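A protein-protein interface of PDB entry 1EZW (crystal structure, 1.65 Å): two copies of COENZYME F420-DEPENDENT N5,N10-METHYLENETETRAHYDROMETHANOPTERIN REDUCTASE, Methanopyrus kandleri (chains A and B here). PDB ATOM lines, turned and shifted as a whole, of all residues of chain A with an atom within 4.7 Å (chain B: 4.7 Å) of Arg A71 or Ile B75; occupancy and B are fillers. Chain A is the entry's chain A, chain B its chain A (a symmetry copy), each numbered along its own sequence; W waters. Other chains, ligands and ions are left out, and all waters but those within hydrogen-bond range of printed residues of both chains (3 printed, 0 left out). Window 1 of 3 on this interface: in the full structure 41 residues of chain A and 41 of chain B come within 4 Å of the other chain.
O of Thr A70 sits at hydrogen-bond distance from N of His B72, at 2.9 Å. N of His A72 sits at hydrogen-bond distance from O of Thr B70, at 2.9 Å. A ring nitrogen (NE2) of His B72 sits at hydrogen-bond distance from the backbone carbonyl oxygen (O) of Met A106 (3.4 Å).
The side-chain hydroxyl (OG1) of Thr A70 is in hydrogen-bond range of the guanidinium group (NH2) of Arg A71 (3.5 Å). The backbone carbonyl oxygen (O) of Arg A71 lies within hydrogen-bond range of the indole nitrogen (NE1) of Trp A117, at 3.4 Å. The backbone carbonyl oxygen of Ile A75 sits close to the side-chain amide oxygen of Asn A79 (3.5 Å). OG1 of Thr B70 sits at hydrogen-bond distance from NH2 of Arg B71. N of Leu B74 lies within hydrogen-bond range of ND1 of His B72 (3.0 Å). O of Ile B75 lies close to OD1 of Asn B79 (3.5 Å).
Leu B74 touches Tyr A40. CD1 of Ile B75 touches CB of Tyr A40, 3.7 Å away. Tyr A40 touches Ser B78. Arg B71 touches Thr A70 (CA to O, 3.4 Å). Arg A71 touches Thr B70 (CA to O, 3.4 Å). Arg A71 touches Ile B75. Ile A75 touches Arg B71 (CG2 to NH1, 3.6 Å). Leu B74 touches Met A106 (CD1 to CA, 3.8 Å). Thr B70 touches Trp A117.
Arg A71 touches two residues of chain B. Ile B75 touches two residues of chain A. Printed residues of chain A within 4 Å of Leu B74: Tyr A40 and Met A106. Printed residues of chain B within 4 Å of Ile A75: Arg B71. The nearest residue of chain A that does not touch Ile B75 is Thr A70 (4.04 Å). The nearest printed residue of chain B that does not touch Ile A75 is Thr B70 (4.04 Å).
Of the 10 printed residues of chain B, 6 touch a printed residue of chain A. Hydrophobic or aromatic side chains of chain B within 4 Å of the printed part of chain A: His B72, Leu B74 and Ile B75. Of the 15 printed residues of chain A, 7 touch a printed residue of chain B. Printed residues of chain A that touch a printed residue of chain B: Tyr A40, Thr A70, Arg A71, His A72, Ile A75, Met A106 and Trp A117. Hydrophobic or aromatic side chains of chain A within 4 Å of the printed part of chain B: Tyr A40, His A72, Ile A75, Met A106 and Trp A117. Among the printed residues, 12 pairs touch across the chains. Among the printed residues, no Asp or Glu carboxylate lies within 4 Å of a Lys or Arg side-chain nitrogen of the other chain.
Thr A70 touches Arg B71, and with the chains exchanged Arg A71 touches Thr B70. Thr A70 touches His B72, and with the chains exchanged His A72 touches Thr B70. Arg A71 touches Ile B75, and with the chains exchanged Ile A75 touches Arg B71.
Water W2 bridges OD1 of Asn A79 (2.6 Å) and NH1 of Arg B71 (2.8 Å). Water W3 lies within hydrogen-bond range of the side-chain amide oxygen of Asn B79 (2.6 Å) and the guanidinium group of Arg A71 (2.8 Å). Water W1 bridges a ring nitrogen (NE2) of His B72 (2.8 Å) and the backbone carbonyl oxygen (O) of Met A106 (2.8 Å).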
ATOM      1  N   ASP A  38      -5.426 -31.793  25.544  1.00  0.00           N
ATOM      2  CA  ASP A  38      -5.493 -31.600  24.099  1.00  0.00           C
ATOM      3  C   ASP A  38      -5.457 -32.918  23.353  1.00  0.00           C
ATOM      4  O   ASP A  38      -4.363 -33.421  23.047  1.00  0.00           O
ATOM      5  CB  ASP A  38      -4.315 -30.677  23.656  1.00  0.00           C
ATOM      6  CG  ASP A  38      -4.150 -30.607  22.143  1.00  0.00           C
ATOM      7  OD1 ASP A  38      -5.192 -30.643  21.470  1.00  0.00           O
ATOM      8  OD2 ASP A  38      -2.998 -30.511  21.660  1.00  0.00           O
ATOM      9  N   TYR A  40      -7.447 -34.970  20.012  1.00  0.00           N
ATOM     10  CA  TYR A  40      -8.347 -34.752  18.879  1.00  0.00           C
ATOM     11  C   TYR A  40      -9.730 -35.364  19.087  1.00  0.00           C
ATOM     12  O   TYR A  40     -10.720 -34.889  18.508  1.00  0.00           O
ATOM     13  CB  TYR A  40      -7.722 -35.341  17.584  1.00  0.00           C
ATOM     14  CG  TYR A  40      -7.962 -36.832  17.503  1.00  0.00           C
ATOM     15  CD1 TYR A  40      -9.157 -37.327  16.960  1.00  0.00           C
ATOM     16  CD2 TYR A  40      -7.125 -37.727  18.209  1.00  0.00           C
ATOM     17  CE1 TYR A  40      -9.550 -38.653  17.142  1.00  0.00           C
ATOM     18  CE2 TYR A  40      -7.513 -39.073  18.394  1.00  0.00           C
ATOM     19  CZ  TYR A  40      -8.717 -39.518  17.880  1.00  0.00           C
ATOM     20  OH  TYR A  40      -9.169 -40.791  18.182  1.00  0.00           O
ATOM     21  N   TYR A  45      -9.184 -27.762  22.665  1.00  0.00           N
ATOM     22  CA  TYR A  45      -8.789 -26.957  23.814  1.00  0.00           C
ATOM     23  C   TYR A  45      -9.018 -25.478  23.556  1.00  0.00           C
ATOM     24  O   TYR A  45      -9.392 -24.763  24.490  1.00  0.00           O
ATOM     25  CB  TYR A  45      -7.334 -27.246  24.263  1.00  0.00           C
ATOM     26  CG  TYR A  45      -6.207 -26.573  23.480  1.00  0.00           C
ATOM     27  CD1 TYR A  45      -5.921 -25.194  23.620  1.00  0.00           C
ATOM     28  CD2 TYR A  45      -5.423 -27.321  22.623  1.00  0.00           C
ATOM     29  CE1 TYR A  45      -4.903 -24.603  22.942  1.00  0.00           C
ATOM     30  CE2 TYR A  45      -4.365 -26.733  21.918  1.00  0.00           C
ATOM     31  CZ  TYR A  45      -4.114 -25.386  22.084  1.00  0.00           C
ATOM     32  OH  TYR A  45      -3.090 -24.795  21.433  1.00  0.00           O
ATOM     33  N   THR A  66      -0.431 -29.731  25.477  1.00  0.00           N
ATOM     34  CA  THR A  66      -0.488 -29.866  24.040  1.00  0.00           C
ATOM     35  C   THR A  66       0.846 -30.432  23.586  1.00  0.00           C
ATOM     36  O   THR A  66       1.570 -30.956  24.412  1.00  0.00           O
ATOM     37  CB  THR A  66      -0.894 -28.546  23.357  1.00  0.00           C
ATOM     38  OG1 THR A  66      -1.008 -28.797  21.941  1.00  0.00           O
ATOM     39  CG2 THR A  66       0.093 -27.408  23.635  1.00  0.00           C
ATOM     40  N   PRO A  68       4.203 -30.616  20.238  1.00  0.00           N
ATOM     41  CA  PRO A  68       4.827 -29.972  19.053  1.00  0.00           C
ATOM     42  C   PRO A  68       4.410 -30.470  17.687  1.00  0.00           C
ATOM     43  O   PRO A  68       4.759 -29.842  16.683  1.00  0.00           O
ATOM     44  CB  PRO A  68       6.325 -30.319  19.218  1.00  0.00           C
ATOM     45  CG  PRO A  68       6.453 -30.750  20.689  1.00  0.00           C
ATOM     46  CD  PRO A  68       5.170 -31.482  20.951  1.00  0.00           C
ATOM     47  N   TYR A  69       3.674 -31.574  17.647  1.00  0.00           N
ATOM     48  CA  TYR A  69       3.424 -32.278  16.396  1.00  0.00           C
ATOM     49  C   TYR A  69       2.143 -32.121  15.631  1.00  0.00           C
ATOM     50  O   TYR A  69       2.157 -32.073  14.406  1.00  0.00           O
ATOM     51  CB  TYR A  69       3.602 -33.788  16.637  1.00  0.00           C
ATOM     52  CG  TYR A  69       4.904 -34.114  17.360  1.00  0.00           C
ATOM     53  CD1 TYR A  69       4.888 -34.505  18.705  1.00  0.00           C
ATOM     54  CD2 TYR A  69       6.147 -33.913  16.736  1.00  0.00           C
ATOM     55  CE1 TYR A  69       6.063 -34.689  19.418  1.00  0.00           C
ATOM     56  CE2 TYR A  69       7.365 -34.097  17.470  1.00  0.00           C
ATOM     57  CZ  TYR A  69       7.295 -34.484  18.811  1.00  0.00           C
ATOM     58  OH  TYR A  69       8.458 -34.682  19.573  1.00  0.00           O
ATOM     59  N   THR A  70       1.020 -32.094  16.341  1.00  0.00           N
ATOM     60  CA  THR A  70      -0.247 -32.068  15.627  1.00  0.00           C
ATOM     61  C   THR A  70      -0.622 -30.704  15.062  1.00  0.00           C
ATOM     62  O   THR A  70      -1.612 -30.607  14.335  1.00  0.00           O
ATOM     63  CB  THR A  70      -1.378 -32.564  16.518  1.00  0.00           C
ATOM     64  OG1 THR A  70      -1.513 -31.635  17.603  1.00  0.00           O
ATOM     65  CG2 THR A  70      -1.079 -34.034  17.061  1.00  0.00           C
ATOM     66  N   ARG A  71       0.125 -29.657  15.422  1.00  0.00           N
ATOM     67  CA  ARG A  71      -0.123 -28.306  14.877  1.00  0.00           C
ATOM     68  C   ARG A  71       1.247 -27.680  14.730  1.00  0.00           C
ATOM     69  O   ARG A  71       2.141 -27.941  15.531  1.00  0.00           O
ATOM     70  CB  ARG A  71      -0.887 -27.423  15.878  1.00  0.00           C
ATOM     71  CG  ARG A  71      -2.258 -27.965  16.255  1.00  0.00           C
ATOM     72  CD  ARG A  71      -2.864 -26.960  17.271  1.00  0.00           C
ATOM     73  NE  ARG A  71      -4.149 -27.411  17.821  1.00  0.00           N
ATOM     74  CZ  ARG A  71      -4.258 -28.379  18.730  1.00  0.00           C
ATOM     75  NH1 ARG A  71      -5.448 -28.753  19.196  1.00  0.00           N
ATOM     76  NH2 ARG A  71      -3.161 -28.981  19.170  1.00  0.00           N
ATOM     77  N   HIS A  72       1.419 -26.817  13.731  1.00  0.00           N
ATOM     78  CA  HIS A  72       2.683 -26.124  13.562  1.00  0.00           C
ATOM     79  C   HIS A  72       2.910 -25.263  14.808  1.00  0.00           C
ATOM     80  O   HIS A  72       1.970 -24.697  15.365  1.00  0.00           O
ATOM     81  CB  HIS A  72       2.583 -25.231  12.319  1.00  0.00           C
ATOM     82  CG  HIS A  72       3.894 -24.675  11.852  1.00  0.00           C
ATOM     83  ND1 HIS A  72       4.550 -23.659  12.507  1.00  0.00           N
ATOM     84  CD2 HIS A  72       4.675 -25.014  10.791  1.00  0.00           C
ATOM     85  CE1 HIS A  72       5.691 -23.393  11.873  1.00  0.00           C
ATOM     86  NE2 HIS A  72       5.784 -24.201  10.825  1.00  0.00           N
ATOM     87  N   PRO A  73       4.146 -25.162  15.292  1.00  0.00           N
ATOM     88  CA  PRO A  73       4.357 -24.341  16.474  1.00  0.00           C
ATOM     89  C   PRO A  73       3.916 -22.885  16.361  1.00  0.00           C
ATOM     90  O   PRO A  73       3.578 -22.278  17.373  1.00  0.00           O
ATOM     91  CB  PRO A  73       5.862 -24.526  16.757  1.00  0.00           C
ATOM     92  CG  PRO A  73       6.427 -24.885  15.449  1.00  0.00           C
ATOM     93  CD  PRO A  73       5.409 -25.851  14.916  1.00  0.00           C
ATOM     94  N   ILE A  75       1.219 -21.989  14.860  1.00  0.00           N
ATOM     95  CA  ILE A  75      -0.232 -22.053  15.118  1.00  0.00           C
ATOM     96  C   ILE A  75      -0.452 -22.177  16.652  1.00  0.00           C
ATOM     97  O   ILE A  75      -1.336 -21.518  17.229  1.00  0.00           O
ATOM     98  CB  ILE A  75      -0.861 -23.214  14.373  1.00  0.00           C
ATOM     99  CG1 ILE A  75      -0.852 -22.899  12.864  1.00  0.00           C
ATOM    100  CG2 ILE A  75      -2.291 -23.475  14.877  1.00  0.00           C
ATOM    101  CD1 ILE A  75      -1.668 -21.646  12.502  1.00  0.00           C
ATOM    102  N   THR A  76       0.334 -23.017  17.317  1.00  0.00           N
ATOM    103  CA  THR A  76       0.203 -23.097  18.776  1.00  0.00           C
ATOM    104  C   THR A  76       0.494 -21.711  19.391  1.00  0.00           C
ATOM    105  O   THR A  76      -0.227 -21.260  20.281  1.00  0.00           O
ATOM    106  CB  THR A  76       1.184 -24.166  19.334  1.00  0.00           C
ATOM    107  OG1 THR A  76       0.758 -25.458  18.884  1.00  0.00           O
ATOM    108  CG2 THR A  76       1.194 -24.119  20.875  1.00  0.00           C
ATOM    109  N   ASN A  79      -2.515 -19.555  18.994  1.00  0.00           N
ATOM    110  CA  ASN A  79      -3.567 -19.991  19.946  1.00  0.00           C
ATOM    111  C   ASN A  79      -3.306 -19.402  21.328  1.00  0.00           C
ATOM    112  O   ASN A  79      -4.199 -18.810  21.935  1.00  0.00           O
ATOM    113  CB  ASN A  79      -3.617 -21.502  20.112  1.00  0.00           C
ATOM    114  CG  ASN A  79      -4.144 -22.186  18.911  1.00  0.00           C
ATOM    115  OD1 ASN A  79      -4.724 -21.542  18.063  1.00  0.00           O
ATOM    116  ND2 ASN A  79      -3.982 -23.514  18.833  1.00  0.00           N
ATOM    117  N   MET A 106      -4.286 -41.461  15.963  1.00  0.00           N
ATOM    118  CA  MET A 106      -4.143 -40.479  14.884  1.00  0.00           C
ATOM    119  C   MET A 106      -3.347 -40.993  13.699  1.00  0.00           C
ATOM    120  O   MET A 106      -3.511 -40.482  12.596  1.00  0.00           O
ATOM    121  CB  MET A 106      -3.465 -39.213  15.398  1.00  0.00           C
ATOM    122  CG  MET A 106      -4.247 -38.520  16.492  1.00  0.00           C
ATOM    123  SD  MET A 106      -3.499 -36.971  17.006  1.00  0.00           S
ATOM    124  CE  MET A 106      -4.110 -35.872  15.637  1.00  0.00           C
ATOM    125  N   TRP A 117       8.152 -30.179  10.955  1.00  0.00           N
ATOM    126  CA  TRP A 117       8.114 -28.795  10.494  1.00  0.00           C
ATOM    127  C   TRP A 117       9.392 -28.215   9.907  1.00  0.00           C
ATOM    128  O   TRP A 117       9.551 -26.997   9.800  1.00  0.00           O
ATOM    129  CB  TRP A 117       7.558 -27.881  11.601  1.00  0.00           C
ATOM    130  CG  TRP A 117       6.247 -28.388  12.207  1.00  0.00           C
ATOM    131  CD1 TRP A 117       6.046 -28.782  13.508  1.00  0.00           C
ATOM    132  CD2 TRP A 117       4.989 -28.596  11.532  1.00  0.00           C
ATOM    133  NE1 TRP A 117       4.755 -29.218  13.678  1.00  0.00           N
ATOM    134  CE2 TRP A 117       4.087 -29.118  12.488  1.00  0.00           C
ATOM    135  CE3 TRP A 117       4.542 -28.397  10.209  1.00  0.00           C
ATOM    136  CZ2 TRP A 117       2.752 -29.440  12.174  1.00  0.00           C
ATOM    137  CZ3 TRP A 117       3.214 -28.722   9.891  1.00  0.00           C
ATOM    138  CH2 TRP A 117       2.334 -29.237  10.884  1.00  0.00           C
ATOM    139  N   THR B  70      -1.224 -27.247   8.220  1.00  0.00           N
ATOM    140  CA  THR B  70      -0.688 -26.720   9.466  1.00  0.00           C
ATOM    141  C   THR B  70      -1.261 -27.369  10.719  1.00  0.00           C
ATOM    142  O   THR B  70      -0.779 -27.081  11.817  1.00  0.00           O
ATOM    143  CB  THR B  70      -0.895 -25.214   9.548  1.00  0.00           C
ATOM    144  OG1 THR B  70      -2.309 -24.974   9.589  1.00  0.00           O
ATOM    145  CG2 THR B  70      -0.228 -24.474   8.302  1.00  0.00           C
ATOM    146  N   ARG B  71      -2.299 -28.196  10.571  1.00  0.00           N
ATOM    147  CA  ARG B  71      -2.881 -28.919  11.721  1.00  0.00           C
ATOM    148  C   ARG B  71      -3.295 -30.268  11.172  1.00  0.00           C
ATOM    149  O   ARG B  71      -3.705 -30.373  10.018  1.00  0.00           O
ATOM    150  CB  ARG B  71      -4.174 -28.249  12.215  1.00  0.00           C
ATOM    151  CG  ARG B  71      -3.980 -26.817  12.694  1.00  0.00           C
ATOM    152  CD  ARG B  71      -5.379 -26.309  13.136  1.00  0.00           C
ATOM    153  NE  ARG B  71      -5.375 -24.890  13.517  1.00  0.00           N
ATOM    154  CZ  ARG B  71      -5.302 -23.895  12.634  1.00  0.00           C
ATOM    155  NH1 ARG B  71      -5.301 -22.624  13.032  1.00  0.00           N
ATOM    156  NH2 ARG B  71      -5.226 -24.179  11.341  1.00  0.00           N
ATOM    157  N   HIS B  72      -3.232 -31.308  12.001  1.00  0.00           N
ATOM    158  CA  HIS B  72      -3.674 -32.623  11.571  1.00  0.00           C
ATOM    159  C   HIS B  72      -5.167 -32.528  11.246  1.00  0.00           C
ATOM    160  O   HIS B  72      -5.916 -31.817  11.917  1.00  0.00           O
ATOM    161  CB  HIS B  72      -3.451 -33.609  12.724  1.00  0.00           C
ATOM    162  CG  HIS B  72      -3.589 -35.051  12.339  1.00  0.00           C
ATOM    163  ND1 HIS B  72      -4.805 -35.644  12.091  1.00  0.00           N
ATOM    164  CD2 HIS B  72      -2.647 -36.013  12.147  1.00  0.00           C
ATOM    165  CE1 HIS B  72      -4.611 -36.917  11.754  1.00  0.00           C
ATOM    166  NE2 HIS B  72      -3.307 -37.164  11.787  1.00  0.00           N
ATOM    167  N   PRO B  73      -5.634 -33.209  10.202  1.00  0.00           N
ATOM    168  CA  PRO B  73      -7.053 -33.117   9.899  1.00  0.00           C
ATOM    169  C   PRO B  73      -8.002 -33.524  11.022  1.00  0.00           C
ATOM    170  O   PRO B  73      -9.123 -33.028  11.072  1.00  0.00           O
ATOM    171  CB  PRO B  73      -7.187 -33.968   8.619  1.00  0.00           C
ATOM    172  CG  PRO B  73      -6.049 -34.895   8.689  1.00  0.00           C
ATOM    173  CD  PRO B  73      -4.937 -34.001   9.153  1.00  0.00           C
ATOM    174  N   LEU B  74      -7.553 -34.385  11.953  1.00  0.00           N
ATOM    175  CA  LEU B  74      -8.411 -34.786  13.059  1.00  0.00           C
ATOM    176  C   LEU B  74      -8.527 -33.602  14.029  1.00  0.00           C
ATOM    177  O   LEU B  74      -9.533 -33.477  14.711  1.00  0.00           O
ATOM    178  CB  LEU B  74      -7.835 -36.005  13.812  1.00  0.00           C
ATOM    179  CG  LEU B  74      -8.028 -37.322  13.039  1.00  0.00           C
ATOM    180  CD1 LEU B  74      -7.212 -38.452  13.748  1.00  0.00           C
ATOM    181  CD2 LEU B  74      -9.536 -37.699  13.002  1.00  0.00           C
ATOM    182  N   ILE B  75      -7.478 -32.778  14.105  1.00  0.00           N
ATOM    183  CA  ILE B  75      -7.543 -31.569  14.948  1.00  0.00           C
ATOM    184  C   ILE B  75      -8.506 -30.552  14.274  1.00  0.00           C
ATOM    185  O   ILE B  75      -9.338 -29.915  14.945  1.00  0.00           O
ATOM    186  CB  ILE B  75      -6.162 -30.976  15.146  1.00  0.00           C
ATOM    187  CG1 ILE B  75      -5.343 -31.916  16.054  1.00  0.00           C
ATOM    188  CG2 ILE B  75      -6.256 -29.564  15.750  1.00  0.00           C
ATOM    189  CD1 ILE B  75      -5.956 -32.091  17.454  1.00  0.00           C
ATOM    190  N   THR B  76      -8.400 -30.386  12.961  1.00  0.00           N
ATOM    191  CA  THR B  76      -9.346 -29.492  12.286  1.00  0.00           C
ATOM    192  C   THR B  76     -10.784 -30.012  12.504  1.00  0.00           C
ATOM    193  O   THR B  76     -11.691 -29.233  12.797  1.00  0.00           O
ATOM    194  CB  THR B  76      -9.010 -29.417  10.769  1.00  0.00           C
ATOM    195  OG1 THR B  76      -7.748 -28.757  10.612  1.00  0.00           O
ATOM    196  CG2 THR B  76     -10.112 -28.640  10.022  1.00  0.00           C
ATOM    197  N   ALA B  77     -11.011 -31.337  12.376  1.00  0.00           N
ATOM    198  CA  ALA B  77     -12.348 -31.888  12.601  1.00  0.00           C
ATOM    199  C   ALA B  77     -12.861 -31.521  14.017  1.00  0.00           C
ATOM    200  O   ALA B  77     -14.014 -31.105  14.195  1.00  0.00           O
ATOM    201  CB  ALA B  77     -12.329 -33.416  12.430  1.00  0.00           C
ATOM    202  N   SER B  78     -12.018 -31.772  15.019  1.00  0.00           N
ATOM    203  CA  SER B  78     -12.374 -31.424  16.385  1.00  0.00           C
ATOM    204  C   SER B  78     -12.743 -29.929  16.495  1.00  0.00           C
ATOM    205  O   SER B  78     -13.776 -29.596  17.129  1.00  0.00           O
ATOM    206  CB  SER B  78     -11.189 -31.731  17.329  1.00  0.00           C
ATOM    207  OG  SER B  78     -11.497 -31.315  18.672  1.00  0.00           O
ATOM    208  N   ASN B  79     -11.918 -29.039  15.914  1.00  0.00           N
ATOM    209  CA  ASN B  79     -12.214 -27.584  15.942  1.00  0.00           C
ATOM    210  C   ASN B  79     -13.608 -27.318  15.383  1.00  0.00           C
ATOM    211  O   ASN B  79     -14.412 -26.627  16.010  1.00  0.00           O
ATOM    212  CB  ASN B  79     -11.239 -26.771  15.103  1.00  0.00           C
ATOM    213  CG  ASN B  79      -9.890 -26.709  15.706  1.00  0.00           C
ATOM    214  OD1 ASN B  79      -9.739 -27.029  16.867  1.00  0.00           O
ATOM    215  ND2 ASN B  79      -8.888 -26.260  14.938  1.00  0.00           N
HETATM  216  O   HOH W   1      -1.720 -39.253  10.822  1.00  0.00           O
HETATM  217  O   HOH W   2      -5.000 -21.286  15.506  1.00  0.00           O
HETATM  218  O   HOH W   3      -8.138 -28.286  18.460  1.00  0.00           O
